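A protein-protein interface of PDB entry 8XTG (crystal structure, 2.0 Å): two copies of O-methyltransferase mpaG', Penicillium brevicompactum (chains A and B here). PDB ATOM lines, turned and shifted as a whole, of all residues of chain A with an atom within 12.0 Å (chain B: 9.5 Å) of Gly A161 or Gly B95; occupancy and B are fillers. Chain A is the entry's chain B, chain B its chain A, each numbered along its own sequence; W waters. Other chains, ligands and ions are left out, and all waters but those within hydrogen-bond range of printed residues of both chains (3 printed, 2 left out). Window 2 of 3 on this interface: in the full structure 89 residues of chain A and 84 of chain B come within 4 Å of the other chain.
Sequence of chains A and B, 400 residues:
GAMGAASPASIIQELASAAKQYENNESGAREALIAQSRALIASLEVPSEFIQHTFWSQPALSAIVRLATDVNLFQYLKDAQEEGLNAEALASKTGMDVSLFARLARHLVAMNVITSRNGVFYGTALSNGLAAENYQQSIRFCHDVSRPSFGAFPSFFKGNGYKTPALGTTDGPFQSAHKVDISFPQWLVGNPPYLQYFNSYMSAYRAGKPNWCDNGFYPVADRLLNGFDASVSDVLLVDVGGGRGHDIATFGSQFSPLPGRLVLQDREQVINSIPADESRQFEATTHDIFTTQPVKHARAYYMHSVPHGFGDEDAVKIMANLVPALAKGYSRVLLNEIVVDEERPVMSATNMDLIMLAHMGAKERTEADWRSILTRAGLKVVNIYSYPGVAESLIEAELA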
ATOM      1  N   ALA A 152     -24.914 -18.033  16.820  1.00  0.00           N
ATOM      2  CA  ALA A 152     -23.613 -17.390  16.703  1.00  0.00           C
ATOM      3  C   ALA A 152     -22.594 -18.225  15.939  1.00  0.00           C
ATOM      4  O   ALA A 152     -21.519 -17.703  15.623  1.00  0.00           O
ATOM      5  CB  ALA A 152     -23.056 -17.068  18.093  1.00  0.00           C
ATOM      6  N   PHE A 153     -22.895 -19.491  15.639  1.00  0.00           N
ATOM      7  CA  PHE A 153     -21.923 -20.363  14.975  1.00  0.00           C
ATOM      8  C   PHE A 153     -21.305 -19.752  13.724  1.00  0.00           C
ATOM      9  O   PHE A 153     -20.067 -19.724  13.634  1.00  0.00           O
ATOM     10  CB  PHE A 153     -22.558 -21.717  14.620  1.00  0.00           C
ATOM     11  CG  PHE A 153     -22.424 -22.762  15.692  1.00  0.00           C
ATOM     12  CD1 PHE A 153     -22.524 -22.423  17.033  1.00  0.00           C
ATOM     13  CD2 PHE A 153     -22.207 -24.089  15.357  1.00  0.00           C
ATOM     14  CE1 PHE A 153     -22.420 -23.392  18.018  1.00  0.00           C
ATOM     15  CE2 PHE A 153     -22.093 -25.065  16.337  1.00  0.00           C
ATOM     16  CZ  PHE A 153     -22.198 -24.716  17.668  1.00  0.00           C
ATOM     17  N   PRO A 154     -22.070 -19.257  12.739  1.00  0.00           N
ATOM     18  CA  PRO A 154     -21.417 -18.787  11.502  1.00  0.00           C
ATOM     19  C   PRO A 154     -20.465 -17.623  11.720  1.00  0.00           C
ATOM     20  O   PRO A 154     -19.378 -17.606  11.131  1.00  0.00           O
ATOM     21  CB  PRO A 154     -22.601 -18.403  10.600  1.00  0.00           C
ATOM     22  CG  PRO A 154     -23.787 -19.115  11.190  1.00  0.00           C
ATOM     23  CD  PRO A 154     -23.537 -19.122  12.659  1.00  0.00           C
ATOM     24  N   SER A 155     -20.830 -16.652  12.561  1.00  0.00           N
ATOM     25  CA  SER A 155     -19.946 -15.511  12.783  1.00  0.00           C
ATOM     26  C   SER A 155     -18.801 -15.853  13.731  1.00  0.00           C
ATOM     27  O   SER A 155     -17.678 -15.377  13.541  1.00  0.00           O
ATOM     28  CB  SER A 155     -20.744 -14.313  13.310  1.00  0.00           C
ATOM     29  OG  SER A 155     -21.239 -14.552  14.614  1.00  0.00           O
ATOM     30  N   PHE A 156     -19.054 -16.673  14.754  1.00  0.00           N
ATOM     31  CA  PHE A 156     -17.987 -17.021  15.687  1.00  0.00           C
ATOM     32  C   PHE A 156     -16.866 -17.774  14.984  1.00  0.00           C
ATOM     33  O   PHE A 156     -15.692 -17.399  15.087  1.00  0.00           O
ATOM     34  CB  PHE A 156     -18.522 -17.857  16.850  1.00  0.00           C
ATOM     35  CG  PHE A 156     -17.436 -18.392  17.742  1.00  0.00           C
ATOM     36  CD1 PHE A 156     -16.721 -17.541  18.573  1.00  0.00           C
ATOM     37  CD2 PHE A 156     -17.103 -19.737  17.725  1.00  0.00           C
ATOM     38  CE1 PHE A 156     -15.707 -18.024  19.381  1.00  0.00           C
ATOM     39  CE2 PHE A 156     -16.088 -20.225  18.532  1.00  0.00           C
ATOM     40  CZ  PHE A 156     -15.392 -19.367  19.362  1.00  0.00           C
ATOM     41  N   PHE A 157     -17.205 -18.848  14.268  1.00  0.00           N
ATOM     42  CA  PHE A 157     -16.161 -19.657  13.653  1.00  0.00           C
ATOM     43  C   PHE A 157     -15.494 -18.921  12.498  1.00  0.00           C
ATOM     44  O   PHE A 157     -14.307 -19.139  12.231  1.00  0.00           O
ATOM     45  CB  PHE A 157     -16.735 -21.007  13.221  1.00  0.00           C
ATOM     46  CG  PHE A 157     -16.958 -21.950  14.375  1.00  0.00           C
ATOM     47  CD1 PHE A 157     -15.883 -22.421  15.113  1.00  0.00           C
ATOM     48  CD2 PHE A 157     -18.239 -22.327  14.747  1.00  0.00           C
ATOM     49  CE1 PHE A 157     -16.075 -23.269  16.187  1.00  0.00           C
ATOM     50  CE2 PHE A 157     -18.444 -23.176  15.822  1.00  0.00           C
ATOM     51  CZ  PHE A 157     -17.356 -23.648  16.544  1.00  0.00           C
ATOM     52  N   LYS A 158     -16.225 -18.030  11.824  1.00  0.00           N
ATOM     53  CA  LYS A 158     -15.583 -17.118  10.882  1.00  0.00           C
ATOM     54  C   LYS A 158     -14.596 -16.202  11.599  1.00  0.00           C
ATOM     55  O   LYS A 158     -13.498 -15.933  11.090  1.00  0.00           O
ATOM     56  CB  LYS A 158     -16.645 -16.307  10.146  1.00  0.00           C
ATOM     57  CG  LYS A 158     -16.126 -15.495   8.975  1.00  0.00           C
ATOM     58  CD  LYS A 158     -16.769 -14.123   8.970  1.00  0.00           C
ATOM     59  CE  LYS A 158     -17.631 -13.942   7.734  1.00  0.00           C
ATOM     60  NZ  LYS A 158     -18.046 -12.526   7.513  1.00  0.00           N
ATOM     61  N   GLY A 159     -14.961 -15.734  12.799  1.00  0.00           N
ATOM     62  CA  GLY A 159     -14.087 -14.889  13.592  1.00  0.00           C
ATOM     63  C   GLY A 159     -12.909 -15.594  14.235  1.00  0.00           C
ATOM     64  O   GLY A 159     -11.895 -14.944  14.502  1.00  0.00           O
ATOM     65  N   ASN A 160     -13.010 -16.899  14.498  1.00  0.00           N
ATOM     66  CA  ASN A 160     -11.910 -17.646  15.103  1.00  0.00           C
ATOM     67  C   ASN A 160     -11.104 -18.452  14.085  1.00  0.00           C
ATOM     68  O   ASN A 160     -10.249 -19.254  14.475  1.00  0.00           O
ATOM     69  CB  ASN A 160     -12.440 -18.529  16.252  1.00  0.00           C
ATOM     70  CG  ASN A 160     -12.814 -19.955  15.827  1.00  0.00           C
ATOM     71  OD1 ASN A 160     -13.110 -20.231  14.667  1.00  0.00           O
ATOM     72  ND2 ASN A 160     -12.830 -20.864  16.801  1.00  0.00           N
ATOM     73  N   GLY A 161     -11.337 -18.235  12.792  1.00  0.00           N
ATOM     74  CA  GLY A 161     -10.583 -18.926  11.765  1.00  0.00           C
ATOM     75  C   GLY A 161     -11.032 -20.341  11.492  1.00  0.00           C
ATOM     76  O   GLY A 161     -10.254 -21.129  10.947  1.00  0.00           O
ATOM     77  N   TYR A 162     -12.269 -20.686  11.860  1.00  0.00           N
ATOM     78  CA  TYR A 162     -12.827 -22.026  11.662  1.00  0.00           C
ATOM     79  C   TYR A 162     -11.984 -23.082  12.370  1.00  0.00           C
ATOM     80  O   TYR A 162     -11.604 -24.103  11.793  1.00  0.00           O
ATOM     81  CB  TYR A 162     -12.987 -22.339  10.173  1.00  0.00           C
ATOM     82  CG  TYR A 162     -13.995 -21.431   9.510  1.00  0.00           C
ATOM     83  CD1 TYR A 162     -15.356 -21.593   9.741  1.00  0.00           C
ATOM     84  CD2 TYR A 162     -13.587 -20.393   8.679  1.00  0.00           C
ATOM     85  CE1 TYR A 162     -16.286 -20.757   9.150  1.00  0.00           C
ATOM     86  CE2 TYR A 162     -14.511 -19.554   8.083  1.00  0.00           C
ATOM     87  CZ  TYR A 162     -15.857 -19.740   8.324  1.00  0.00           C
ATOM     88  OH  TYR A 162     -16.779 -18.911   7.733  1.00  0.00           O
ATOM     89  N   LYS A 163     -11.702 -22.827  13.645  1.00  0.00           N
ATOM     90  CA  LYS A 163     -10.934 -23.724  14.494  1.00  0.00           C
ATOM     91  C   LYS A 163     -11.839 -24.372  15.532  1.00  0.00           C
ATOM     92  O   LYS A 163     -12.843 -23.792  15.959  1.00  0.00           O
ATOM     93  CB  LYS A 163      -9.805 -22.985  15.220  1.00  0.00           C
ATOM     94  CG  LYS A 163      -8.873 -22.195  14.335  1.00  0.00           C
ATOM     95  CD  LYS A 163      -8.075 -23.113  13.432  1.00  0.00           C
ATOM     96  CE  LYS A 163      -6.756 -22.479  13.036  1.00  0.00           C
ATOM     97  NZ  LYS A 163      -6.428 -22.778  11.616  1.00  0.00           N
ATOM     98  N   THR A 164     -11.469 -25.581  15.930  1.00  0.00           N
ATOM     99  CA  THR A 164     -12.020 -26.153  17.146  1.00  0.00           C
ATOM    100  C   THR A 164     -11.637 -25.263  18.327  1.00  0.00           C
ATOM    101  O   THR A 164     -10.517 -24.737  18.364  1.00  0.00           O
ATOM    102  CB  THR A 164     -11.482 -27.571  17.356  1.00  0.00           C
ATOM    103  OG1 THR A 164     -11.982 -28.424  16.319  1.00  0.00           O
ATOM    104  CG2 THR A 164     -11.910 -28.126  18.709  1.00  0.00           C
ATOM    105  N   PRO A 165     -12.551 -25.025  19.285  1.00  0.00           N
ATOM    106  CA  PRO A 165     -12.155 -24.322  20.512  1.00  0.00           C
ATOM    107  C   PRO A 165     -10.923 -24.948  21.146  1.00  0.00           C
ATOM    108  O   PRO A 165     -10.906 -26.145  21.455  1.00  0.00           O
ATOM    109  CB  PRO A 165     -13.395 -24.458  21.400  1.00  0.00           C
ATOM    110  CG  PRO A 165     -14.521 -24.429  20.414  1.00  0.00           C
ATOM    111  CD  PRO A 165     -14.014 -25.207  19.211  1.00  0.00           C
ATOM    112  N   ALA A 166      -9.873 -24.142  21.311  1.00  0.00           N
ATOM    113  CA  ALA A 166      -8.601 -24.669  21.795  1.00  0.00           C
ATOM    114  C   ALA A 166      -8.678 -25.016  23.275  1.00  0.00           C
ATOM    115  O   ALA A 166      -8.342 -26.134  23.681  1.00  0.00           O
ATOM    116  CB  ALA A 166      -7.484 -23.659  21.532  1.00  0.00           C
ATOM    117  N   ASP A 171     -13.414 -20.578  25.383  1.00  0.00           N
ATOM    118  CA  ASP A 171     -13.195 -19.987  24.067  1.00  0.00           C
ATOM    119  C   ASP A 171     -14.059 -20.691  23.024  1.00  0.00           C
ATOM    120  O   ASP A 171     -13.593 -21.080  21.952  1.00  0.00           O
ATOM    121  CB  ASP A 171     -11.711 -20.025  23.693  1.00  0.00           C
ATOM    122  CG  ASP A 171     -11.126 -21.424  23.745  1.00  0.00           C
ATOM    123  OD1 ASP A 171     -11.864 -22.373  24.081  1.00  0.00           O
ATOM    124  OD2 ASP A 171      -9.922 -21.575  23.440  1.00  0.00           O
ATOM    125  N   GLY A 172     -15.342 -20.856  23.336  1.00  0.00           N
ATOM    126  CA  GLY A 172     -16.280 -21.454  22.418  1.00  0.00           C
ATOM    127  C   GLY A 172     -17.403 -20.504  22.052  1.00  0.00           C
ATOM    128  O   GLY A 172     -17.459 -19.363  22.523  1.00  0.00           O
ATOM    129  N   PRO A 173     -18.324 -20.955  21.192  1.00  0.00           N
ATOM    130  CA  PRO A 173     -19.416 -20.066  20.759  1.00  0.00           C
ATOM    131  C   PRO A 173     -20.361 -19.658  21.879  1.00  0.00           C
ATOM    132  O   PRO A 173     -21.090 -18.671  21.710  1.00  0.00           O
ATOM    133  CB  PRO A 173     -20.144 -20.887  19.681  1.00  0.00           C
ATOM    134  CG  PRO A 173     -19.702 -22.297  19.886  1.00  0.00           C
ATOM    135  CD  PRO A 173     -18.320 -22.234  20.460  1.00  0.00           C
ATOM    136  N   SER A 176     -19.148 -16.156  23.076  1.00  0.00           N
ATOM    137  CA  SER A 176     -19.386 -15.085  22.111  1.00  0.00           C
ATOM    138  C   SER A 176     -20.856 -14.682  22.066  1.00  0.00           C
ATOM    139  O   SER A 176     -21.174 -13.486  22.013  1.00  0.00           O
ATOM    140  CB  SER A 176     -18.901 -15.532  20.729  1.00  0.00           C
ATOM    141  OG  SER A 176     -19.150 -14.547  19.742  1.00  0.00           O
ATOM    142  N   LEU A 357     -20.403 -28.583  21.744  1.00  0.00           N
ATOM    143  CA  LEU A 357     -19.692 -27.448  21.166  1.00  0.00           C
ATOM    144  C   LEU A 357     -20.357 -26.132  21.544  1.00  0.00           C
ATOM    145  O   LEU A 357     -19.677 -25.150  21.866  1.00  0.00           O
ATOM    146  CB  LEU A 357     -19.625 -27.606  19.643  1.00  0.00           C
ATOM    147  CG  LEU A 357     -18.738 -26.667  18.816  1.00  0.00           C
ATOM    148  CD1 LEU A 357     -17.313 -26.639  19.354  1.00  0.00           C
ATOM    149  CD2 LEU A 357     -18.741 -27.065  17.337  1.00  0.00           C
ATOM    150  N   LEU B  67     -23.393 -21.188   7.727  1.00  0.00           N
ATOM    151  CA  LEU B  67     -21.936 -21.176   7.669  1.00  0.00           C
ATOM    152  C   LEU B  67     -21.440 -21.703   6.329  1.00  0.00           C
ATOM    153  O   LEU B  67     -20.459 -21.192   5.775  1.00  0.00           O
ATOM    154  CB  LEU B  67     -21.366 -22.003   8.828  1.00  0.00           C
ATOM    155  CG  LEU B  67     -19.848 -22.196   8.942  1.00  0.00           C
ATOM    156  CD1 LEU B  67     -19.430 -22.159  10.411  1.00  0.00           C
ATOM    157  CD2 LEU B  67     -19.378 -23.495   8.280  1.00  0.00           C
ATOM    158  N   ASP B  70     -20.603 -19.357   3.694  1.00  0.00           N
ATOM    159  CA  ASP B  70     -19.401 -18.553   3.887  1.00  0.00           C
ATOM    160  C   ASP B  70     -18.132 -19.247   3.409  1.00  0.00           C
ATOM    161  O   ASP B  70     -17.103 -18.578   3.265  1.00  0.00           O
ATOM    162  CB  ASP B  70     -19.215 -18.187   5.369  1.00  0.00           C
ATOM    163  CG  ASP B  70     -20.302 -17.267   5.902  1.00  0.00           C
ATOM    164  OD1 ASP B  70     -20.895 -16.502   5.115  1.00  0.00           O
ATOM    165  OD2 ASP B  70     -20.562 -17.304   7.126  1.00  0.00           O
ATOM    166  N   VAL B  71     -18.169 -20.563   3.183  1.00  0.00           N
ATOM    167  CA  VAL B  71     -16.960 -21.324   2.865  1.00  0.00           C
ATOM    168  C   VAL B  71     -17.137 -22.173   1.607  1.00  0.00           C
ATOM    169  O   VAL B  71     -16.348 -23.094   1.360  1.00  0.00           O
ATOM    170  CB  VAL B  71     -16.536 -22.212   4.052  1.00  0.00           C
ATOM    171  CG1 VAL B  71     -16.197 -21.365   5.268  1.00  0.00           C
ATOM    172  CG2 VAL B  71     -17.635 -23.212   4.390  1.00  0.00           C
ATOM    173  N   ASN B  72     -18.169 -21.884   0.809  1.00  0.00           N
ATOM    174  CA  ASN B  72     -18.333 -22.469  -0.525  1.00  0.00           C
ATOM    175  C   ASN B  72     -18.593 -23.978  -0.481  1.00  0.00           C
ATOM    176  O   ASN B  72     -18.307 -24.688  -1.451  1.00  0.00           O
ATOM    177  CB  ASN B  72     -17.112 -22.169  -1.408  1.00  0.00           C
ATOM    178  CG  ASN B  72     -17.477 -21.912  -2.855  1.00  0.00           C
ATOM    179  OD1 ASN B  72     -18.352 -21.102  -3.153  1.00  0.00           O
ATOM    180  ND2 ASN B  72     -16.800 -22.604  -3.766  1.00  0.00           N
ATOM    181  N   LEU B  73     -19.159 -24.472   0.626  1.00  0.00           N
ATOM    182  CA  LEU B  73     -19.299 -25.914   0.835  1.00  0.00           C
ATOM    183  C   LEU B  73     -20.140 -26.574  -0.257  1.00  0.00           C
ATOM    184  O   LEU B  73     -19.700 -27.532  -0.902  1.00  0.00           O
ATOM    185  CB  LEU B  73     -19.909 -26.185   2.211  1.00  0.00           C
ATOM    186  CG  LEU B  73     -20.247 -27.651   2.505  1.00  0.00           C
ATOM    187  CD1 LEU B  73     -19.012 -28.531   2.379  1.00  0.00           C
ATOM    188  CD2 LEU B  73     -20.862 -27.796   3.885  1.00  0.00           C
ATOM    189  N   TYR B  76     -18.421 -26.717  -3.635  1.00  0.00           N
ATOM    190  CA  TYR B  76     -17.355 -27.712  -3.739  1.00  0.00           C
ATOM    191  C   TYR B  76     -17.926 -29.114  -3.914  1.00  0.00           C
ATOM    192  O   TYR B  76     -17.423 -29.899  -4.728  1.00  0.00           O
ATOM    193  CB  TYR B  76     -16.441 -27.663  -2.511  1.00  0.00           C
ATOM    194  CG  TYR B  76     -15.624 -26.396  -2.402  1.00  0.00           C
ATOM    195  CD1 TYR B  76     -15.045 -25.821  -3.527  1.00  0.00           C
ATOM    196  CD2 TYR B  76     -15.440 -25.769  -1.175  1.00  0.00           C
ATOM    197  CE1 TYR B  76     -14.302 -24.656  -3.433  1.00  0.00           C
ATOM    198  CE2 TYR B  76     -14.699 -24.604  -1.070  1.00  0.00           C
ATOM    199  CZ  TYR B  76     -14.133 -24.051  -2.202  1.00  0.00           C
ATOM    200  OH  TYR B  76     -13.395 -22.891  -2.104  1.00  0.00           O
ATOM    201  N   ALA B  87     -13.256 -35.613   4.366  1.00  0.00           N
ATOM    202  CA  ALA B  87     -13.212 -34.486   5.291  1.00  0.00           C
ATOM    203  C   ALA B  87     -11.926 -33.686   5.131  1.00  0.00           C
ATOM    204  O   ALA B  87     -11.950 -32.450   5.181  1.00  0.00           O
ATOM    205  CB  ALA B  87     -13.366 -34.979   6.730  1.00  0.00           C
ATOM    206  N   GLU B  88     -10.794 -34.371   4.935  1.00  0.00           N
ATOM    207  CA  GLU B  88      -9.524 -33.677   4.758  1.00  0.00           C
ATOM    208  C   GLU B  88      -9.521 -32.831   3.489  1.00  0.00           C
ATOM    209  O   GLU B  88      -8.985 -31.717   3.479  1.00  0.00           O
ATOM    210  CB  GLU B  88      -8.374 -34.688   4.726  1.00  0.00           C
ATOM    211  CG  GLU B  88      -7.005 -34.070   4.474  1.00  0.00           C
ATOM    212  CD  GLU B  88      -6.176 -33.935   5.735  1.00  0.00           C
ATOM    213  OE1 GLU B  88      -5.803 -34.979   6.312  1.00  0.00           O
ATOM    214  OE2 GLU B  88      -5.906 -32.790   6.154  1.00  0.00           O
ATOM    215  N   ALA B  89     -10.107 -33.347   2.405  1.00  0.00           N
ATOM    216  CA  ALA B  89     -10.143 -32.588   1.157  1.00  0.00           C
ATOM    217  C   ALA B  89     -11.045 -31.367   1.275  1.00  0.00           C
ATOM    218  O   ALA B  89     -10.698 -30.283   0.788  1.00  0.00           O
ATOM    219  CB  ALA B  89     -10.594 -33.486   0.004  1.00  0.00           C
ATOM    220  N   LEU B  90     -12.200 -31.515   1.925  1.00  0.00           N
ATOM    221  CA  LEU B  90     -13.111 -30.386   2.074  1.00  0.00           C
ATOM    222  C   LEU B  90     -12.605 -29.373   3.096  1.00  0.00           C
ATOM    223  O   LEU B  90     -12.815 -28.168   2.923  1.00  0.00           O
ATOM    224  CB  LEU B  90     -14.499 -30.888   2.463  1.00  0.00           C
ATOM    225  CG  LEU B  90     -15.433 -31.217   1.300  1.00  0.00           C
ATOM    226  CD1 LEU B  90     -16.512 -32.203   1.736  1.00  0.00           C
ATOM    227  CD2 LEU B  90     -16.049 -29.943   0.727  1.00  0.00           C
ATOM    228  N   ALA B  91     -11.949 -29.837   4.163  1.00  0.00           N
ATOM    229  CA  ALA B  91     -11.380 -28.913   5.142  1.00  0.00           C
ATOM    230  C   ALA B  91     -10.324 -28.021   4.505  1.00  0.00           C
ATOM    231  O   ALA B  91     -10.235 -26.829   4.820  1.00  0.00           O
ATOM    232  CB  ALA B  91     -10.777 -29.689   6.313  1.00  0.00           C
ATOM    233  N   SER B  92      -9.512 -28.587   3.614  1.00  0.00           N
ATOM    234  CA  SER B  92      -8.533 -27.795   2.882  1.00  0.00           C
ATOM    235  C   SER B  92      -9.221 -26.773   1.986  1.00  0.00           C
ATOM    236  O   SER B  92      -8.874 -25.587   1.996  1.00  0.00           O
ATOM    237  CB  SER B  92      -7.629 -28.723   2.065  1.00  0.00           C
ATOM    238  OG  SER B  92      -6.986 -28.030   1.008  1.00  0.00           O
ATOM    239  N   LYS B  93     -10.218 -27.217   1.214  1.00  0.00           N
ATOM    240  CA  LYS B  93     -10.892 -26.328   0.270  1.00  0.00           C
ATOM    241  C   LYS B  93     -11.630 -25.197   0.981  1.00  0.00           C
ATOM    242  O   LYS B  93     -11.699 -24.075   0.465  1.00  0.00           O
ATOM    243  CB  LYS B  93     -11.865 -27.128  -0.599  1.00  0.00           C
ATOM    244  CG  LYS B  93     -11.268 -27.645  -1.891  1.00  0.00           C
ATOM    245  CD  LYS B  93     -12.053 -28.839  -2.404  1.00  0.00           C
ATOM    246  CE  LYS B  93     -11.771 -29.088  -3.874  1.00  0.00           C
ATOM    247  NZ  LYS B  93     -11.927 -27.843  -4.677  1.00  0.00           N
ATOM    248  N   THR B  94     -12.204 -25.474   2.151  1.00  0.00           N
ATOM    249  CA  THR B  94     -12.972 -24.473   2.884  1.00  0.00           C
ATOM    250  C   THR B  94     -12.133 -23.656   3.860  1.00  0.00           C
ATOM    251  O   THR B  94     -12.607 -22.621   4.340  1.00  0.00           O
ATOM    252  CB  THR B  94     -14.122 -25.137   3.654  1.00  0.00           C
ATOM    253  OG1 THR B  94     -13.598 -26.150   4.520  1.00  0.00           O
ATOM    254  CG2 THR B  94     -15.127 -25.764   2.699  1.00  0.00           C
ATOM    255  N   GLY B  95     -10.909 -24.083   4.159  1.00  0.00           N
ATOM    256  CA  GLY B  95     -10.086 -23.375   5.120  1.00  0.00           C
ATOM    257  C   GLY B  95     -10.451 -23.651   6.560  1.00  0.00           C
ATOM    258  O   GLY B  95     -10.263 -22.783   7.418  1.00  0.00           O
ATOM    259  N   MET B  96     -10.958 -24.844   6.851  1.00  0.00           N
ATOM    260  CA  MET B  96     -11.516 -25.184   8.149  1.00  0.00           C
ATOM    261  C   MET B  96     -10.658 -26.250   8.814  1.00  0.00           C
ATOM    262  O   MET B  96      -9.991 -27.039   8.138  1.00  0.00           O
ATOM    263  CB  MET B  96     -12.949 -25.702   7.993  1.00  0.00           C
ATOM    264  CG  MET B  96     -13.918 -24.678   7.430  1.00  0.00           C
ATOM    265  SD  MET B  96     -15.598 -25.312   7.256  1.00  0.00           S
ATOM    266  CE  MET B  96     -15.988 -25.748   8.953  1.00  0.00           C
ATOM    267  N   ASP B  97     -10.678 -26.276  10.143  1.00  0.00           N
ATOM    268  CA  ASP B  97     -10.073 -27.395  10.850  1.00  0.00           C
ATOM    269  C   ASP B  97     -10.767 -28.689  10.439  1.00  0.00           C
ATOM    270  O   ASP B  97     -11.993 -28.735  10.302  1.00  0.00           O
ATOM    271  CB  ASP B  97     -10.168 -27.181  12.363  1.00  0.00           C
ATOM    272  CG  ASP B  97      -9.778 -28.418  13.157  1.00  0.00           C
ATOM    273  OD1 ASP B  97      -8.566 -28.724  13.242  1.00  0.00           O
ATOM    274  OD2 ASP B  97     -10.684 -29.072  13.713  1.00  0.00           O
ATOM    275  N   VAL B  98      -9.972 -29.740  10.210  1.00  0.00           N
ATOM    276  CA  VAL B  98     -10.530 -30.999   9.714  1.00  0.00           C
ATOM    277  C   VAL B  98     -11.552 -31.561  10.694  1.00  0.00           C
ATOM    278  O   VAL B  98     -12.611 -32.056  10.291  1.00  0.00           O
ATOM    279  CB  VAL B  98      -9.407 -32.012   9.426  1.00  0.00           C
ATOM    280  CG1 VAL B  98      -9.994 -33.319   8.911  1.00  0.00           C
ATOM    281  CG2 VAL B  98      -8.423 -31.437   8.420  1.00  0.00           C
ATOM    282  N   LEU B 100     -13.330 -29.894  13.136  1.00  0.00           N
ATOM    283  CA  LEU B 100     -14.520 -29.048  13.160  1.00  0.00           C
ATOM    284  C   LEU B 100     -15.383 -29.285  11.931  1.00  0.00           C
ATOM    285  O   LEU B 100     -16.607 -29.416  12.043  1.00  0.00           O
ATOM    286  CB  LEU B 100     -14.130 -27.573  13.257  1.00  0.00           C
ATOM    287  CG  LEU B 100     -15.317 -26.605  13.204  1.00  0.00           C
ATOM    288  CD1 LEU B 100     -16.295 -26.872  14.349  1.00  0.00           C
ATOM    289  CD2 LEU B 100     -14.843 -25.160  13.215  1.00  0.00           C
ATOM    290  N   PHE B 101     -14.764 -29.357  10.748  1.00  0.00           N
ATOM    291  CA  PHE B 101     -15.545 -29.584   9.536  1.00  0.00           C
ATOM    292  C   PHE B 101     -16.262 -30.925   9.584  1.00  0.00           C
ATOM    293  O   PHE B 101     -17.448 -31.019   9.247  1.00  0.00           O
ATOM    294  CB  PHE B 101     -14.672 -29.520   8.283  1.00  0.00           C
ATOM    295  CG  PHE B 101     -15.418 -29.935   7.047  1.00  0.00           C
ATOM    296  CD1 PHE B 101     -16.281 -29.050   6.423  1.00  0.00           C
ATOM    297  CD2 PHE B 101     -15.318 -31.228   6.555  1.00  0.00           C
ATOM    298  CE1 PHE B 101     -17.002 -29.432   5.316  1.00  0.00           C
ATOM    299  CE2 PHE B 101     -16.042 -31.612   5.446  1.00  0.00           C
ATOM    300  CZ  PHE B 101     -16.885 -30.713   4.830  1.00  0.00           C
HETATM  301  O   HOH W   1     -19.858 -13.618   5.283  1.00  0.00           O
HETATM  302  O   HOH W   2      -8.998 -29.938  16.001  1.00  0.00           O
HETATM  303  O   HOH W   3      -8.611 -26.225  15.047  1.00  0.00           O
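The backbone NH (N) of Asp B97 lies within hydrogen-bond range of the backbone carbonyl oxygen (O) of Tyr A162 (2.9 Å). The side-chain carboxylate of Asp B97 sits at hydrogen-bond distance from the side-chain hydroxyl of Thr A164, at 3.0 Å.
OD1 of Asn A160 lies close to O of Phe A157, 2.9 Å away. The backbone carbonyl oxygen of Phe A157 lies within hydrogen-bond range of the backbone NH of Tyr A162 (2.6 Å). The backbone NH (N) of Tyr A162 lies within hydrogen-bond range of the side-chain amide oxygen (OD1) of Asn A160, 3.0 Å away.
Phe A157 touches Leu B100. Gly B95 touches Gly A161. Leu B67 touches Tyr A162 (CD1 to CE1, 3.7 Å). Asp B70 touches Tyr A162 (CB to OH, 3.5 Å). Val B71 touches Tyr A162 (CG1 to CZ, 3.5 Å). Met B96 touches Tyr A162. Leu B100 touches Tyr A162. Lys A163 touches Leu B100 (O to CD2, 3.7 Å). CD1 of Leu B100 touches CD2 of Leu A357, 3.9 Å away.
Of the printed residues of chain B, Phe A157 touches Leu B100. No residue of chain B comes within 4 Å of Gly A159. No residue of chain B comes within 4 Å of Asn A160. Of chain B, only Gly B95 comes within 4 Å of Gly A161. Of the printed residues of chain B, Lys A163 touches Leu B100. Printed residues of chain A within 4 Å of Val B71: Tyr A162. Ala B91 touches none of the printed residues of chain A. No residue of chain A comes within 4 Å of Ser B92. No residue of chain A comes within 4 Å of Thr B94. Of chain A, only Tyr A162 (3.7 Å) comes within 4 Å of Met B96. Printed residues of chain A within 4 Å of Asp B97: Tyr A162 (2.9 Å) and Thr A164 (3.0 Å). The nearest residue of chain B that does not touch Gly A161 is Met B96 (5.1 Å).
Of the 20 printed residues of chain A, 6 touch a printed residue of chain B. Hydrophobic or aromatic side chains of chain A that line the printed part of chain B: Phe A157, Tyr A162 and Leu A357. Of the 20 printed residues of chain B, 7 touch a printed residue of chain A. Printed residues of chain B that touch a printed residue of chain A: Leu B67, Asp B70, Val B71, Gly B95, Met B96, Asp B97 and Leu B100. Hydrophobic or aromatic side chains of chain B that line the printed part of chain A: Leu B67, Val B71, Met B96 and Leu B100. Among the printed residues, 13 pairs touch across the chains.
No position is printed for both chains. Of the 13 pairs that touch across the chains among the printed residues, none has its exchanged pair printed and touching as well.
Water W2 lies within hydrogen-bond range of the side-chain carboxylate of Asp B97 (3.0 Å) and the side-chain hydroxyl of Thr A164 (3.4 Å). Water W3 lies within hydrogen-bond range of the backbone NH of Thr A164 (3.1 Å) and the side-chain carboxylate of Asp B97 (3.1 Å). Water W1 bridges OD1 of Asp B70 (3.1 Å) and NZ of Lys A158 (3.1 Å).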
